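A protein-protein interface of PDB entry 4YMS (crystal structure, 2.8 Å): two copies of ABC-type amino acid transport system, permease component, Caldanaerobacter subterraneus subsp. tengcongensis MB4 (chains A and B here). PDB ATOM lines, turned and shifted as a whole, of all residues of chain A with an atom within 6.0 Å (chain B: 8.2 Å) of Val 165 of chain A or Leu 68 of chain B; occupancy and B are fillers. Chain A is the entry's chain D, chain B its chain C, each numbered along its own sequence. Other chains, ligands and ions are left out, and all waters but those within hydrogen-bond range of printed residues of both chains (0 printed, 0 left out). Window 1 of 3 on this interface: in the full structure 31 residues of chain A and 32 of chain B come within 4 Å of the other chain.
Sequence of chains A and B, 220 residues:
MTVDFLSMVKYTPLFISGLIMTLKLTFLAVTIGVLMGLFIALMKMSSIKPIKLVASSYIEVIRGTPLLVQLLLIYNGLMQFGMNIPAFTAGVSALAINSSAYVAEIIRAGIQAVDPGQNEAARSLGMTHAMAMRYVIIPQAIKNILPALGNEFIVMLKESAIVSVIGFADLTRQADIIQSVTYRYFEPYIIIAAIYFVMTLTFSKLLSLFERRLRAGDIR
Among the printed residues, pairs that only touch across the chains: Ala 161 of chain A with Leu 68 of chain B (3.1 Å), Leu 68 of chain A with Ser 164 of chain B (3.4 Å), Thr 172 of chain A with Val 69 of chain B (3.6 Å), Ser 164 of chain A with Leu 68 of chain B (3.6 Å), Val 165 of chain A with Val 165 of chain B (3.6 Å) and Val 165 of chain A with Leu 68 of chain B (3.96 Å).
Val 165 of chain A touches just these residues of chain B: Leu 68 (3.96 Å) and Val 165 (3.6 Å).
Printed residues of chain A within 4 Å of Leu 68 of chain B: Ala 161, Ser 164 and Val 165.
Of chain B, only Leu 68 comes within 4 Å of Ser 164 of chain A.
Of the printed residues of chain B, Thr 172 of chain A touches Val 69.
Of the printed residues of chain B, Ala 161 of chain A touches Leu 68.
Printed residues of chain B within 4 Å of Leu 68 of chain A: Ser 164 (3.4 Å).
Thr 65 of chain B touches none of the printed residues of chain A.
The nearest printed residue of chain B that does not touch Ala 161 of chain A is Pro 66 of chain B (4.1 Å).
Of the 21 printed residues of chain B, 4 touch a printed residue of chain A.
Hydrophobic or aromatic side chains of chain B that line the printed part of chain A: Leu 68, Val 69 and Val 165.
Among the printed residues, no Asp or Glu carboxylate lies within 4 Å of a Lys or Arg side-chain nitrogen of the other chain.
Leu 68 of chain A touches Ser 164 of chain B, and with the chains exchanged Ser 164 of chain A touches Leu 68 of chain B.
Val 165 of chain A touches Leu 68 of chain B, but with the chains exchanged Leu 68 of chain A does not touch Val 165 of chain B (4.1 Å).
Val 165 of chain B touches its own counterpart, Val 165 of chain A.
Of the 6 pairs that touch across the chains among the printed residues, 3 have their exchanged pair printed and touching as well.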
ATOM      1  N   LEU A  68       1.321  14.916  32.428  1.00  0.00           N
ATOM      2  CA  LEU A  68       0.432  16.075  32.494  1.00  0.00           C
ATOM      3  C   LEU A  68      -0.693  15.824  33.480  1.00  0.00           C
ATOM      4  O   LEU A  68      -0.827  16.549  34.477  1.00  0.00           O
ATOM      5  CB  LEU A  68      -0.160  16.399  31.118  1.00  0.00           C
ATOM      6  CG  LEU A  68      -0.287  17.865  30.685  1.00  0.00           C
ATOM      7  CD1 LEU A  68      -1.610  18.136  29.977  1.00  0.00           C
ATOM      8  CD2 LEU A  68      -0.097  18.814  31.846  1.00  0.00           C
ATOM      9  N   LEU A  71       0.348  16.078  36.936  1.00  0.00           N
ATOM     10  CA  LEU A  71       0.647  17.468  37.286  1.00  0.00           C
ATOM     11  C   LEU A  71      -0.635  18.204  37.681  1.00  0.00           C
ATOM     12  O   LEU A  71      -0.792  18.675  38.818  1.00  0.00           O
ATOM     13  CB  LEU A  71       1.317  18.194  36.108  1.00  0.00           C
ATOM     14  CG  LEU A  71       2.493  19.160  36.328  1.00  0.00           C
ATOM     15  CD1 LEU A  71       2.446  20.320  35.332  1.00  0.00           C
ATOM     16  CD2 LEU A  71       2.585  19.663  37.763  1.00  0.00           C
ATOM     17  N   LEU A  72      -1.560  18.256  36.727  1.00  0.00           N
ATOM     18  CA  LEU A  72      -2.834  18.931  36.901  1.00  0.00           C
ATOM     19  C   LEU A  72      -3.620  18.317  38.064  1.00  0.00           C
ATOM     20  O   LEU A  72      -4.280  19.033  38.812  1.00  0.00           O
ATOM     21  CB  LEU A  72      -3.629  18.873  35.593  1.00  0.00           C
ATOM     22  CG  LEU A  72      -2.827  19.453  34.417  1.00  0.00           C
ATOM     23  CD1 LEU A  72      -3.600  19.504  33.103  1.00  0.00           C
ATOM     24  CD2 LEU A  72      -2.272  20.831  34.762  1.00  0.00           C
ATOM     25  N   ALA A 161       9.965  20.625  31.305  1.00  0.00           N
ATOM     26  CA  ALA A 161       9.460  21.745  30.508  1.00  0.00           C
ATOM     27  C   ALA A 161       7.928  21.810  30.515  1.00  0.00           C
ATOM     28  O   ALA A 161       7.343  22.733  29.946  1.00  0.00           O
ATOM     29  CB  ALA A 161       9.975  21.668  29.066  1.00  0.00           C
ATOM     30  N   ILE A 162       7.283  20.797  31.087  1.00  0.00           N
ATOM     31  CA  ILE A 162       5.832  20.727  31.107  1.00  0.00           C
ATOM     32  C   ILE A 162       5.258  21.572  32.233  1.00  0.00           C
ATOM     33  O   ILE A 162       4.046  21.728  32.338  1.00  0.00           O
ATOM     34  CB  ILE A 162       5.325  19.289  31.249  1.00  0.00           C
ATOM     35  CG1 ILE A 162       3.926  19.163  30.643  1.00  0.00           C
ATOM     36  CG2 ILE A 162       5.378  18.830  32.705  1.00  0.00           C
ATOM     37  CD1 ILE A 162       3.267  17.854  30.956  1.00  0.00           C
ATOM     38  N   VAL A 163       6.110  22.073  33.116  1.00  0.00           N
ATOM     39  CA  VAL A 163       5.616  22.915  34.203  1.00  0.00           C
ATOM     40  C   VAL A 163       5.387  24.353  33.736  1.00  0.00           C
ATOM     41  O   VAL A 163       4.922  25.201  34.492  1.00  0.00           O
ATOM     42  CB  VAL A 163       6.577  22.917  35.407  1.00  0.00           C
ATOM     43  CG1 VAL A 163       6.952  21.488  35.770  1.00  0.00           C
ATOM     44  CG2 VAL A 163       7.822  23.750  35.100  1.00  0.00           C
ATOM     45  N   SER A 164       5.698  24.635  32.482  1.00  0.00           N
ATOM     46  CA  SER A 164       5.425  25.958  31.978  1.00  0.00           C
ATOM     47  C   SER A 164       3.908  26.147  31.941  1.00  0.00           C
ATOM     48  O   SER A 164       3.402  27.177  32.394  1.00  0.00           O
ATOM     49  CB  SER A 164       6.047  26.162  30.596  1.00  0.00           C
ATOM     50  OG  SER A 164       5.253  25.550  29.606  1.00  0.00           O
ATOM     51  N   VAL A 165       3.178  25.124  31.495  1.00  0.00           N
ATOM     52  CA  VAL A 165       1.730  25.253  31.326  1.00  0.00           C
ATOM     53  C   VAL A 165       0.999  25.522  32.644  1.00  0.00           C
ATOM     54  O   VAL A 165      -0.163  25.938  32.652  1.00  0.00           O
ATOM     55  CB  VAL A 165       1.117  23.989  30.684  1.00  0.00           C
ATOM     56  CG1 VAL A 165       1.981  23.514  29.532  1.00  0.00           C
ATOM     57  CG2 VAL A 165       0.958  22.901  31.709  1.00  0.00           C
ATOM     58  N   ILE A 166       1.710  25.331  33.750  1.00  0.00           N
ATOM     59  CA  ILE A 166       1.168  25.516  35.084  1.00  0.00           C
ATOM     60  C   ILE A 166       1.544  26.925  35.539  1.00  0.00           C
ATOM     61  O   ILE A 166       1.143  27.395  36.614  1.00  0.00           O
ATOM     62  CB  ILE A 166       1.737  24.450  36.044  1.00  0.00           C
ATOM     63  CG1 ILE A 166       0.712  23.961  37.053  1.00  0.00           C
ATOM     64  CG2 ILE A 166       2.983  24.948  36.778  1.00  0.00           C
ATOM     65  CD1 ILE A 166       1.365  23.109  38.175  1.00  0.00           C
ATOM     66  N   GLY A 167       2.340  27.590  34.708  1.00  0.00           N
ATOM     67  CA  GLY A 167       2.787  28.934  35.006  1.00  0.00           C
ATOM     68  C   GLY A 167       4.058  29.030  35.834  1.00  0.00           C
ATOM     69  O   GLY A 167       4.264  30.018  36.537  1.00  0.00           O
ATOM     70  N   PHE A 168       4.883  27.986  35.810  1.00  0.00           N
ATOM     71  CA  PHE A 168       6.182  28.028  36.482  1.00  0.00           C
ATOM     72  C   PHE A 168       7.207  28.652  35.538  1.00  0.00           C
ATOM     73  O   PHE A 168       7.219  28.341  34.344  1.00  0.00           O
ATOM     74  CB  PHE A 168       6.626  26.629  36.909  1.00  0.00           C
ATOM     75  CG  PHE A 168       7.858  26.620  37.774  1.00  0.00           C
ATOM     76  CD1 PHE A 168       7.766  26.870  39.141  1.00  0.00           C
ATOM     77  CD2 PHE A 168       9.117  26.392  37.214  1.00  0.00           C
ATOM     78  CE1 PHE A 168       8.897  26.876  39.936  1.00  0.00           C
ATOM     79  CE2 PHE A 168      10.257  26.401  37.999  1.00  0.00           C
ATOM     80  CZ  PHE A 168      10.148  26.646  39.366  1.00  0.00           C
ATOM     81  N   THR A 172      11.225  27.142  29.491  1.00  0.00           N
ATOM     82  CA  THR A 172      10.257  27.189  28.396  1.00  0.00           C
ATOM     83  C   THR A 172       9.299  28.372  28.574  1.00  0.00           C
ATOM     84  O   THR A 172       8.836  28.981  27.599  1.00  0.00           O
ATOM     85  CB  THR A 172       9.451  25.887  28.302  1.00  0.00           C
ATOM     86  OG1 THR A 172      10.348  24.791  28.098  1.00  0.00           O
ATOM     87  CG2 THR A 172       8.466  25.946  27.148  1.00  0.00           C
ATOM     88  N   THR B  65      15.417  16.937  22.845  1.00  0.00           N
ATOM     89  CA  THR B  65      14.656  18.176  22.998  1.00  0.00           C
ATOM     90  C   THR B  65      13.178  17.875  23.301  1.00  0.00           C
ATOM     91  O   THR B  65      12.628  16.883  22.806  1.00  0.00           O
ATOM     92  CB  THR B  65      14.828  19.035  21.720  1.00  0.00           C
ATOM     93  OG1 THR B  65      15.399  20.301  22.061  1.00  0.00           O
ATOM     94  CG2 THR B  65      13.531  19.185  20.923  1.00  0.00           C
ATOM     95  N   PRO B  66      12.542  18.699  24.157  1.00  0.00           N
ATOM     96  CA  PRO B  66      11.203  18.356  24.669  1.00  0.00           C
ATOM     97  C   PRO B  66      10.101  18.313  23.612  1.00  0.00           C
ATOM     98  O   PRO B  66      10.200  18.993  22.595  1.00  0.00           O
ATOM     99  CB  PRO B  66      10.931  19.456  25.702  1.00  0.00           C
ATOM    100  CG  PRO B  66      12.283  19.972  26.093  1.00  0.00           C
ATOM    101  CD  PRO B  66      13.083  19.902  24.818  1.00  0.00           C
ATOM    102  N   LEU B  67       9.101  17.460  23.819  1.00  0.00           N
ATOM    103  CA  LEU B  67       7.932  17.410  22.945  1.00  0.00           C
ATOM    104  C   LEU B  67       7.152  18.754  23.008  1.00  0.00           C
ATOM    105  O   LEU B  67       6.729  19.277  21.968  1.00  0.00           O
ATOM    106  CB  LEU B  67       7.032  16.234  23.335  1.00  0.00           C
ATOM    107  CG  LEU B  67       6.119  15.522  22.328  1.00  0.00           C
ATOM    108  CD1 LEU B  67       4.836  15.118  23.024  1.00  0.00           C
ATOM    109  CD2 LEU B  67       5.817  16.328  21.093  1.00  0.00           C
ATOM    110  N   LEU B  68       6.970  19.304  24.219  1.00  0.00           N
ATOM    111  CA  LEU B  68       6.246  20.569  24.384  1.00  0.00           C
ATOM    112  C   LEU B  68       6.812  21.645  23.472  1.00  0.00           C
ATOM    113  O   LEU B  68       6.117  22.148  22.591  1.00  0.00           O
ATOM    114  CB  LEU B  68       6.313  21.077  25.822  1.00  0.00           C
ATOM    115  CG  LEU B  68       5.034  21.669  26.435  1.00  0.00           C
ATOM    116  CD1 LEU B  68       5.323  22.606  27.607  1.00  0.00           C
ATOM    117  CD2 LEU B  68       4.135  22.330  25.401  1.00  0.00           C
ATOM    118  N   VAL B  69       8.090  21.955  23.663  1.00  0.00           N
ATOM    119  CA  VAL B  69       8.763  22.997  22.900  1.00  0.00           C
ATOM    120  C   VAL B  69       8.619  22.782  21.384  1.00  0.00           C
ATOM    121  O   VAL B  69       8.555  23.743  20.625  1.00  0.00           O
ATOM    122  CB  VAL B  69      10.245  23.091  23.312  1.00  0.00           C
ATOM    123  CG1 VAL B  69      11.004  24.068  22.442  1.00  0.00           C
ATOM    124  CG2 VAL B  69      10.343  23.497  24.787  1.00  0.00           C
ATOM    125  N   GLN B  70       8.531  21.534  20.935  1.00  0.00           N
ATOM    126  CA  GLN B  70       8.288  21.276  19.511  1.00  0.00           C
ATOM    127  C   GLN B  70       6.856  21.662  19.133  1.00  0.00           C
ATOM    128  O   GLN B  70       6.615  22.241  18.055  1.00  0.00           O
ATOM    129  CB  GLN B  70       8.551  19.809  19.172  1.00  0.00           C
ATOM    130  CG  GLN B  70       9.999  19.407  19.381  1.00  0.00           C
ATOM    131  CD  GLN B  70      10.197  17.898  19.513  1.00  0.00           C
ATOM    132  OE1 GLN B  70      11.040  17.445  20.290  1.00  0.00           O
ATOM    133  NE2 GLN B  70       9.428  17.120  18.745  1.00  0.00           N
ATOM    134  N   LEU B  71       5.911  21.307  20.009  1.00  0.00           N
ATOM    135  CA  LEU B  71       4.503  21.656  19.824  1.00  0.00           C
ATOM    136  C   LEU B  71       4.351  23.178  19.699  1.00  0.00           C
ATOM    137  O   LEU B  71       3.867  23.688  18.686  1.00  0.00           O
ATOM    138  CB  LEU B  71       3.646  21.131  20.985  1.00  0.00           C
ATOM    139  CG  LEU B  71       2.271  20.531  20.654  1.00  0.00           C
ATOM    140  CD1 LEU B  71       1.253  20.792  21.754  1.00  0.00           C
ATOM    141  CD2 LEU B  71       1.748  20.998  19.295  1.00  0.00           C
ATOM    142  N   LEU B  72       4.780  23.891  20.738  1.00  0.00           N
ATOM    143  CA  LEU B  72       4.684  25.336  20.758  1.00  0.00           C
ATOM    144  C   LEU B  72       5.465  25.972  19.607  1.00  0.00           C
ATOM    145  O   LEU B  72       5.012  26.950  19.014  1.00  0.00           O
ATOM    146  CB  LEU B  72       5.157  25.885  22.103  1.00  0.00           C
ATOM    147  CG  LEU B  72       4.386  25.289  23.289  1.00  0.00           C
ATOM    148  CD1 LEU B  72       4.724  25.942  24.644  1.00  0.00           C
ATOM    149  CD2 LEU B  72       2.889  25.303  23.044  1.00  0.00           C
ATOM    150  N   LEU B  73       6.615  25.410  19.264  1.00  0.00           N
ATOM    151  CA  LEU B  73       7.358  25.923  18.126  1.00  0.00           C
ATOM    152  C   LEU B  73       6.501  25.833  16.884  1.00  0.00           C
ATOM    153  O   LEU B  73       6.546  26.720  16.040  1.00  0.00           O
ATOM    154  CB  LEU B  73       8.662  25.162  17.890  1.00  0.00           C
ATOM    155  CG  LEU B  73       9.429  25.801  16.733  1.00  0.00           C
ATOM    156  CD1 LEU B  73       9.957  27.162  17.167  1.00  0.00           C
ATOM    157  CD2 LEU B  73      10.536  24.935  16.182  1.00  0.00           C
ATOM    158  N   ILE B  74       5.716  24.773  16.741  1.00  0.00           N
ATOM    159  CA  ILE B  74       4.876  24.728  15.550  1.00  0.00           C
ATOM    160  C   ILE B  74       3.706  25.715  15.659  1.00  0.00           C
ATOM    161  O   ILE B  74       3.483  26.546  14.774  1.00  0.00           O
ATOM    162  CB  ILE B  74       4.345  23.311  15.270  1.00  0.00           C
ATOM    163  CG1 ILE B  74       5.506  22.408  14.863  1.00  0.00           C
ATOM    164  CG2 ILE B  74       3.321  23.338  14.145  1.00  0.00           C
ATOM    165  CD1 ILE B  74       5.090  21.048  14.349  1.00  0.00           C
ATOM    166  N   TYR B  75       3.007  25.671  16.781  1.00  0.00           N
ATOM    167  CA  TYR B  75       1.790  26.443  16.949  1.00  0.00           C
ATOM    168  C   TYR B  75       2.099  27.929  17.080  1.00  0.00           C
ATOM    169  O   TYR B  75       1.833  28.714  16.173  1.00  0.00           O
ATOM    170  CB  TYR B  75       1.056  25.940  18.182  1.00  0.00           C
ATOM    171  CG  TYR B  75      -0.380  26.367  18.358  1.00  0.00           C
ATOM    172  CD1 TYR B  75      -0.760  27.160  19.441  1.00  0.00           C
ATOM    173  CD2 TYR B  75      -1.370  25.916  17.490  1.00  0.00           C
ATOM    174  CE1 TYR B  75      -2.081  27.521  19.638  1.00  0.00           C
ATOM    175  CE2 TYR B  75      -2.694  26.266  17.681  1.00  0.00           C
ATOM    176  CZ  TYR B  75      -3.045  27.073  18.755  1.00  0.00           C
ATOM    177  OH  TYR B  75      -4.357  27.427  18.940  1.00  0.00           O
ATOM    178  N   ASN B  76       2.691  28.304  18.206  1.00  0.00           N
ATOM    179  CA  ASN B  76       3.014  29.692  18.481  1.00  0.00           C
ATOM    180  C   ASN B  76       4.138  30.280  17.639  1.00  0.00           C
ATOM    181  O   ASN B  76       4.010  31.374  17.098  1.00  0.00           O
ATOM    182  CB  ASN B  76       3.371  29.828  19.944  1.00  0.00           C
ATOM    183  CG  ASN B  76       2.230  29.449  20.828  1.00  0.00           C
ATOM    184  OD1 ASN B  76       1.127  29.202  20.338  1.00  0.00           O
ATOM    185  ND2 ASN B  76       2.459  29.433  22.138  1.00  0.00           N
ATOM    186  N   ALA B  94       3.641  17.732  15.519  1.00  0.00           N
ATOM    187  CA  ALA B  94       4.615  17.580  16.592  1.00  0.00           C
ATOM    188  C   ALA B  94       4.857  16.096  16.916  1.00  0.00           C
ATOM    189  O   ALA B  94       6.006  15.636  16.922  1.00  0.00           O
ATOM    190  CB  ALA B  94       4.165  18.340  17.837  1.00  0.00           C
ATOM    191  N   LEU B  95       3.779  15.352  17.155  1.00  0.00           N
ATOM    192  CA  LEU B  95       3.872  13.938  17.514  1.00  0.00           C
ATOM    193  C   LEU B  95       4.482  13.091  16.395  1.00  0.00           C
ATOM    194  O   LEU B  95       5.360  12.273  16.643  1.00  0.00           O
ATOM    195  CB  LEU B  95       2.497  13.374  17.894  1.00  0.00           C
ATOM    196  CG  LEU B  95       1.841  13.729  19.237  1.00  0.00           C
ATOM    197  CD1 LEU B  95       0.606  12.861  19.457  1.00  0.00           C
ATOM    198  CD2 LEU B  95       2.783  13.636  20.438  1.00  0.00           C
ATOM    199  N   ASN B  98       8.289  13.792  16.504  1.00  0.00           N
ATOM    200  CA  ASN B  98       8.921  13.160  17.667  1.00  0.00           C
ATOM    201  C   ASN B  98       9.012  11.629  17.477  1.00  0.00           C
ATOM    202  O   ASN B  98      10.098  11.001  17.521  1.00  0.00           O
ATOM    203  CB  ASN B  98       8.098  13.557  18.907  1.00  0.00           C
ATOM    204  CG  ASN B  98       8.796  13.276  20.226  1.00  0.00           C
ATOM    205  OD1 ASN B  98       8.419  12.361  20.974  1.00  0.00           O
ATOM    206  ND2 ASN B  98       9.816  14.072  20.528  1.00  0.00           N
ATOM    207  N   GLU B 159       1.650  10.656  25.710  1.00  0.00           N
ATOM    208  CA  GLU B 159       2.263  11.884  25.237  1.00  0.00           C
ATOM    209  C   GLU B 159       1.181  12.855  24.749  1.00  0.00           C
ATOM    210  O   GLU B 159       1.241  14.058  24.994  1.00  0.00           O
ATOM    211  CB  GLU B 159       3.239  11.584  24.091  1.00  0.00           C
ATOM    212  CG  GLU B 159       4.488  10.758  24.431  1.00  0.00           C
ATOM    213  CD  GLU B 159       5.692  11.595  24.858  1.00  0.00           C
ATOM    214  OE1 GLU B 159       5.583  12.333  25.865  1.00  0.00           O
ATOM    215  OE2 GLU B 159       6.748  11.501  24.183  1.00  0.00           O
ATOM    216  N   ILE B 162      -0.699  16.023  25.993  1.00  0.00           N
ATOM    217  CA  ILE B 162      -0.075  17.333  26.108  1.00  0.00           C
ATOM    218  C   ILE B 162      -0.624  18.340  25.111  1.00  0.00           C
ATOM    219  O   ILE B 162      -0.428  19.545  25.272  1.00  0.00           O
ATOM    220  CB  ILE B 162       1.435  17.273  25.910  1.00  0.00           C
ATOM    221  CG1 ILE B 162       2.074  18.481  26.589  1.00  0.00           C
ATOM    222  CG2 ILE B 162       1.792  17.225  24.421  1.00  0.00           C
ATOM    223  CD1 ILE B 162       3.498  18.643  26.231  1.00  0.00           C
ATOM    224  N   VAL B 163      -1.354  17.861  24.109  1.00  0.00           N
ATOM    225  CA  VAL B 163      -1.911  18.770  23.117  1.00  0.00           C
ATOM    226  C   VAL B 163      -3.134  19.443  23.708  1.00  0.00           C
ATOM    227  O   VAL B 163      -3.774  20.267  23.065  1.00  0.00           O
ATOM    228  CB  VAL B 163      -2.323  18.057  21.837  1.00  0.00           C
ATOM    229  CG1 VAL B 163      -1.233  17.099  21.424  1.00  0.00           C
ATOM    230  CG2 VAL B 163      -3.620  17.295  22.068  1.00  0.00           C
ATOM    231  N   SER B 164      -3.471  19.083  24.939  1.00  0.00           N
ATOM    232  CA  SER B 164      -4.573  19.740  25.593  1.00  0.00           C
ATOM    233  C   SER B 164      -4.172  21.189  25.814  1.00  0.00           C
ATOM    234  O   SER B 164      -4.967  22.086  25.565  1.00  0.00           O
ATOM    235  CB  SER B 164      -4.935  19.043  26.902  1.00  0.00           C
ATOM    236  OG  SER B 164      -4.031  19.396  27.930  1.00  0.00           O
ATOM    237  N   VAL B 165      -2.922  21.428  26.215  1.00  0.00           N
ATOM    238  CA  VAL B 165      -2.462  22.787  26.541  1.00  0.00           C
ATOM    239  C   VAL B 165      -2.499  23.752  25.350  1.00  0.00           C
ATOM    240  O   VAL B 165      -2.292  24.954  25.497  1.00  0.00           O
ATOM    241  CB  VAL B 165      -1.028  22.787  27.123  1.00  0.00           C
ATOM    242  CG1 VAL B 165      -0.893  21.730  28.206  1.00  0.00           C
ATOM    243  CG2 VAL B 165       0.008  22.603  26.021  1.00  0.00           C
ATOM    244  N   ILE B 166      -2.733  23.208  24.168  1.00  0.00           N
ATOM    245  CA  ILE B 166      -2.820  23.983  22.943  1.00  0.00           C
ATOM    246  C   ILE B 166      -4.300  24.244  22.646  1.00  0.00           C
ATOM    247  O   ILE B 166      -4.650  24.925  21.683  1.00  0.00           O
ATOM    248  CB  ILE B 166      -2.139  23.221  21.785  1.00  0.00           C
ATOM    249  CG1 ILE B 166      -1.411  24.140  20.818  1.00  0.00           C
ATOM    250  CG2 ILE B 166      -3.129  22.370  21.014  1.00  0.00           C
ATOM    251  CD1 ILE B 166      -0.972  23.379  19.574  1.00  0.00           C
